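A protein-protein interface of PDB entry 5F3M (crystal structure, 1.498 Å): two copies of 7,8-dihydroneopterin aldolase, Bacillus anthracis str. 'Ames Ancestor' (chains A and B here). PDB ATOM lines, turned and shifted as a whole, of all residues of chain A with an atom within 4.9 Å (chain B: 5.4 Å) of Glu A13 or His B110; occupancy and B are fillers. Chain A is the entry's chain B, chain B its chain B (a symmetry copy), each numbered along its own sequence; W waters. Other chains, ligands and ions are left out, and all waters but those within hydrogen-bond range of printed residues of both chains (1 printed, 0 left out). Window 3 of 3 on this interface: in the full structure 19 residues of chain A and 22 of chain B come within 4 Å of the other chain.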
ATOM      1  N   ASP A  11     -26.308  29.316  16.794  1.00  0.00           N
ATOM      2  CA  ASP A  11     -26.914  28.851  15.542  1.00  0.00           C
ATOM      3  C   ASP A  11     -25.995  27.918  14.753  1.00  0.00           C
ATOM      4  O   ASP A  11     -25.841  28.049  13.535  1.00  0.00           O
ATOM      5  CB  ASP A  11     -27.380  30.031  14.683  1.00  0.00           C
ATOM      6  CG  ASP A  11     -28.549  29.675  13.781  1.00  0.00           C
ATOM      7  OD1 ASP A  11     -29.344  28.782  14.151  1.00  0.00           O
ATOM      8  OD2 ASP A  11     -28.688  30.296  12.712  1.00  0.00           O
ATOM      9  N   MET A  12     -25.396  26.952  15.447  1.00  0.00           N
ATOM     10  CA  MET A  12     -24.718  25.868  14.748  1.00  0.00           C
ATOM     11  C   MET A  12     -25.759  25.148  13.909  1.00  0.00           C
ATOM     12  O   MET A  12     -26.884  24.930  14.372  1.00  0.00           O
ATOM     13  CB  MET A  12     -24.116  24.877  15.739  1.00  0.00           C
ATOM     14  CG  MET A  12     -22.916  25.426  16.467  1.00  0.00           C
ATOM     15  SD  MET A  12     -22.392  24.278  17.946  1.00  0.00           S
ATOM     16  CE  MET A  12     -23.587  25.034  19.280  1.00  0.00           C
ATOM     17  N   GLU A  13     -25.413  24.781  12.678  1.00  0.00           N
ATOM     18  CA  GLU A  13     -26.327  24.050  11.810  1.00  0.00           C
ATOM     19  C   GLU A  13     -25.723  22.710  11.428  1.00  0.00           C
ATOM     20  O   GLU A  13     -24.593  22.654  10.928  1.00  0.00           O
ATOM     21  CB  GLU A  13     -26.676  24.827  10.542  1.00  0.00           C
ATOM     22  CG  GLU A  13     -27.765  24.108   9.735  1.00  0.00           C
ATOM     23  CD  GLU A  13     -28.056  24.754   8.393  1.00  0.00           C
ATOM     24  OE1 GLU A  13     -27.360  24.434   7.403  1.00  0.00           O
ATOM     25  OE2 GLU A  13     -28.976  25.591   8.330  1.00  0.00           O
ATOM     26  N   PHE A  14     -26.481  21.641  11.658  1.00  0.00           N
ATOM     27  CA  PHE A  14     -26.064  20.287  11.341  1.00  0.00           C
ATOM     28  C   PHE A  14     -27.155  19.613  10.521  1.00  0.00           C
ATOM     29  O   PHE A  14     -28.321  20.006  10.561  1.00  0.00           O
ATOM     30  CB  PHE A  14     -25.829  19.475  12.625  1.00  0.00           C
ATOM     31  CG  PHE A  14     -24.849  20.117  13.580  1.00  0.00           C
ATOM     32  CD1 PHE A  14     -23.500  20.192  13.263  1.00  0.00           C
ATOM     33  CD2 PHE A  14     -25.278  20.646  14.794  1.00  0.00           C
ATOM     34  CE1 PHE A  14     -22.591  20.784  14.134  1.00  0.00           C
ATOM     35  CE2 PHE A  14     -24.373  21.230  15.679  1.00  0.00           C
ATOM     36  CZ  PHE A  14     -23.027  21.306  15.343  1.00  0.00           C
ATOM     37  N   TYR A  15     -26.772  18.613   9.744  1.00  0.00           N
ATOM     38  CA  TYR A  15     -27.744  17.721   9.125  1.00  0.00           C
ATOM     39  C   TYR A  15     -27.696  16.400   9.877  1.00  0.00           C
ATOM     40  O   TYR A  15     -26.617  15.820  10.046  1.00  0.00           O
ATOM     41  CB  TYR A  15     -27.450  17.505   7.638  1.00  0.00           C
ATOM     42  CG  TYR A  15     -28.646  16.963   6.887  1.00  0.00           C
ATOM     43  CD1 TYR A  15     -29.577  17.826   6.316  1.00  0.00           C
ATOM     44  CD2 TYR A  15     -28.854  15.588   6.764  1.00  0.00           C
ATOM     45  CE1 TYR A  15     -30.691  17.337   5.633  1.00  0.00           C
ATOM     46  CE2 TYR A  15     -29.956  15.089   6.081  1.00  0.00           C
ATOM     47  CZ  TYR A  15     -30.870  15.971   5.519  1.00  0.00           C
ATOM     48  OH  TYR A  15     -31.970  15.498   4.855  1.00  0.00           O
ATOM     49  N   ARG A  30     -32.473  19.347   8.848  1.00  0.00           N
ATOM     50  CA  ARG A  30     -31.643  20.294   9.588  1.00  0.00           C
ATOM     51  C   ARG A  30     -31.886  20.180  11.087  1.00  0.00           C
ATOM     52  O   ARG A  30     -33.023  20.000  11.546  1.00  0.00           O
ATOM     53  CB  ARG A  30     -31.983  21.731   9.195  1.00  0.00           C
ATOM     54  CG  ARG A  30     -31.663  22.113   7.758  1.00  0.00           C
ATOM     55  CD  ARG A  30     -31.972  23.593   7.547  1.00  0.00           C
ATOM     56  NE  ARG A  30     -31.759  24.034   6.165  1.00  0.00           N
ATOM     57  CZ  ARG A  30     -32.732  24.194   5.272  1.00  0.00           C
ATOM     58  NH1 ARG A  30     -34.001  23.949   5.608  1.00  0.00           N
ATOM     59  NH2 ARG A  30     -32.441  24.601   4.041  1.00  0.00           N
ATOM     60  N   PHE A  31     -30.814  20.338  11.853  1.00  0.00           N
ATOM     61  CA  PHE A  31     -30.888  20.595  13.285  1.00  0.00           C
ATOM     62  C   PHE A  31     -29.983  21.776  13.591  1.00  0.00           C
ATOM     63  O   PHE A  31     -28.901  21.905  13.007  1.00  0.00           O
ATOM     64  CB  PHE A  31     -30.444  19.367  14.106  1.00  0.00           C
ATOM     65  CG  PHE A  31     -31.387  18.203  13.990  1.00  0.00           C
ATOM     66  CD1 PHE A  31     -32.411  18.028  14.915  1.00  0.00           C
ATOM     67  CD2 PHE A  31     -31.279  17.308  12.932  1.00  0.00           C
ATOM     68  CE1 PHE A  31     -33.307  16.975  14.793  1.00  0.00           C
ATOM     69  CE2 PHE A  31     -32.165  16.254  12.800  1.00  0.00           C
ATOM     70  CZ  PHE A  31     -33.184  16.079  13.732  1.00  0.00           C
ATOM     71  N   LYS A  32     -30.428  22.643  14.490  1.00  0.00           N
ATOM     72  CA  LYS A  32     -29.627  23.774  14.927  1.00  0.00           C
ATOM     73  C   LYS A  32     -29.406  23.671  16.428  1.00  0.00           C
ATOM     74  O   LYS A  32     -30.223  23.095  17.154  1.00  0.00           O
ATOM     75  CB  LYS A  32     -30.299  25.109  14.574  1.00  0.00           C
ATOM     76  CG  LYS A  32     -30.523  25.323  13.064  1.00  0.00           C
ATOM     77  CD  LYS A  32     -31.378  26.565  12.828  1.00  0.00           C
ATOM     78  CE  LYS A  32     -31.022  27.271  11.524  1.00  0.00           C
ATOM     79  NZ  LYS A  32     -31.166  26.387  10.334  1.00  0.00           N
ATOM     80  N   PHE A  60     -17.569  23.406  19.735  1.00  0.00           N
ATOM     81  CA  PHE A  60     -18.278  23.142  18.483  1.00  0.00           C
ATOM     82  C   PHE A  60     -18.213  21.665  18.113  1.00  0.00           C
ATOM     83  O   PHE A  60     -19.235  21.054  17.771  1.00  0.00           O
ATOM     84  CB  PHE A  60     -17.712  23.975  17.331  1.00  0.00           C
ATOM     85  CG  PHE A  60     -18.295  23.583  15.999  1.00  0.00           C
ATOM     86  CD1 PHE A  60     -19.520  24.098  15.588  1.00  0.00           C
ATOM     87  CD2 PHE A  60     -17.645  22.663  15.185  1.00  0.00           C
ATOM     88  CE1 PHE A  60     -20.081  23.714  14.384  1.00  0.00           C
ATOM     89  CE2 PHE A  60     -18.197  22.274  13.978  1.00  0.00           C
ATOM     90  CZ  PHE A  60     -19.420  22.798  13.578  1.00  0.00           C
ATOM     91  N   PRO B 108     -13.875  24.957  11.065  1.00  0.00           N
ATOM     92  CA  PRO B 108     -14.590  24.266   9.979  1.00  0.00           C
ATOM     93  C   PRO B 108     -15.946  23.777  10.467  1.00  0.00           C
ATOM     94  O   PRO B 108     -16.034  22.969  11.395  1.00  0.00           O
ATOM     95  CB  PRO B 108     -13.660  23.096   9.633  1.00  0.00           C
ATOM     96  CG  PRO B 108     -12.315  23.542  10.099  1.00  0.00           C
ATOM     97  CD  PRO B 108     -12.581  24.321  11.357  1.00  0.00           C
ATOM     98  N   GLY B 109     -17.000  24.268   9.842  1.00  0.00           N
ATOM     99  CA  GLY B 109     -18.348  23.953  10.267  1.00  0.00           C
ATOM    100  C   GLY B 109     -19.288  25.078   9.883  1.00  0.00           C
ATOM    101  O   GLY B 109     -18.906  26.023   9.194  1.00  0.00           O
ATOM    102  N   HIS B 110     -20.528  24.963  10.357  1.00  0.00           N
ATOM    103  CA  HIS B 110     -21.598  25.884   9.987  1.00  0.00           C
ATOM    104  C   HIS B 110     -22.270  26.429  11.239  1.00  0.00           C
ATOM    105  O   HIS B 110     -22.765  25.662  12.067  1.00  0.00           O
ATOM    106  CB  HIS B 110     -22.591  25.169   9.070  1.00  0.00           C
ATOM    107  CG  HIS B 110     -21.933  24.545   7.882  1.00  0.00           C
ATOM    108  ND1 HIS B 110     -21.743  25.222   6.695  1.00  0.00           N
ATOM    109  CD2 HIS B 110     -21.366  23.326   7.717  1.00  0.00           C
ATOM    110  CE1 HIS B 110     -21.114  24.434   5.839  1.00  0.00           C
ATOM    111  NE2 HIS B 110     -20.867  23.282   6.437  1.00  0.00           N
ATOM    112  N   TYR B 111     -22.278  27.753  11.381  1.00  0.00           N
ATOM    113  CA  TYR B 111     -22.722  28.435  12.599  1.00  0.00           C
ATOM    114  C   TYR B 111     -22.834  29.913  12.241  1.00  0.00           C
ATOM    115  O   TYR B 111     -22.346  30.357  11.192  1.00  0.00           O
ATOM    116  CB  TYR B 111     -21.725  28.214  13.771  1.00  0.00           C
ATOM    117  CG  TYR B 111     -20.314  28.383  13.279  1.00  0.00           C
ATOM    118  CD1 TYR B 111     -19.785  29.655  13.051  1.00  0.00           C
ATOM    119  CD2 TYR B 111     -19.535  27.276  12.952  1.00  0.00           C
ATOM    120  CE1 TYR B 111     -18.523  29.824  12.519  1.00  0.00           C
ATOM    121  CE2 TYR B 111     -18.258  27.434  12.428  1.00  0.00           C
ATOM    122  CZ  TYR B 111     -17.762  28.716  12.210  1.00  0.00           C
ATOM    123  OH  TYR B 111     -16.513  28.903  11.671  1.00  0.00           O
ATOM    124  N   ARG B 112     -23.488  30.674  13.116  1.00  0.00           N
ATOM    125  CA  ARG B 112     -23.532  32.120  12.928  1.00  0.00           C
ATOM    126  C   ARG B 112     -22.315  32.819  13.529  1.00  0.00           C
ATOM    127  O   ARG B 112     -21.708  33.672  12.876  1.00  0.00           O
ATOM    128  CB  ARG B 112     -24.821  32.710  13.510  1.00  0.00           C
ATOM    129  CG  ARG B 112     -24.922  34.224  13.299  1.00  0.00           C
ATOM    130  CD  ARG B 112     -26.296  34.792  13.634  1.00  0.00           C
ATOM    131  NE  ARG B 112     -26.482  35.022  15.063  1.00  0.00           N
ATOM    132  CZ  ARG B 112     -27.311  34.320  15.831  1.00  0.00           C
ATOM    133  NH1 ARG B 112     -27.422  34.606  17.122  1.00  0.00           N
ATOM    134  NH2 ARG B 112     -28.033  33.336  15.308  1.00  0.00           N
HETATM  135  O   HOH W   1     -21.723  22.405  11.029  1.00  0.00           O
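O of His B110 is in hydrogen-bond range of N of Glu A13 (2.9 Å).
The side-chain carboxylate (OE2) of Glu A13 lies within salt-bridge range of the guanidinium group (NE) of Arg A30.
NZ of Lys A32 is in salt-bridge range of OE2 of Glu A13.
Asp A11 touches Tyr B111.
Asp A11 touches Arg B112 (CB to NH2, 3.4 Å).
Met A12 touches His B110.
CA of Met A12 touches CA of Tyr B111, at 3.9 Å.
Phe A60 touches Pro B108 (CE2 to O, 3.4 Å).
Gly B109 touches Phe A60 (CA to CZ, 3.7 Å).
Tyr B111 touches Phe A60 (CD2 to CE1, 3.9 Å).
Of chain B, only His B110 comes within 4 Å of Glu A13.
Printed residues of chain B within 4 Å of Met A12: His B110 (3.3 Å) and Tyr B111 (3.9 Å).
Printed residues of chain B within 4 Å of Asp A11: Tyr B111 and Arg B112.
Of the printed residues of chain A, Tyr B111 touches Asp A11 (3.3 Å), Met A12 (3.9 Å) and Phe A60 (3.9 Å).
The nearest residue of chain A that does not touch His B110 is Phe A60 (4.04 Å).
The nearest printed residue of chain B that does not touch Phe A60 is His B110 (4.04 Å).
Hydrophobic or aromatic side chains of chain A that line the printed part of chain B: Met A12 and Phe A60.
Along chain B the printed residues that touch a printed residue of chain A span positions 108 to 112.
Among the printed residues, 8 pairs touch across the chains.
Among the printed residues, no Asp or Glu carboxylate lies within 4 Å of a Lys or Arg side-chain nitrogen of the other chain.
No position is printed for both chains.
Water W1 bridges the backbone carbonyl oxygen of Glu A13 (2.9 Å) and the backbone NH of His B110 (2.9 Å).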
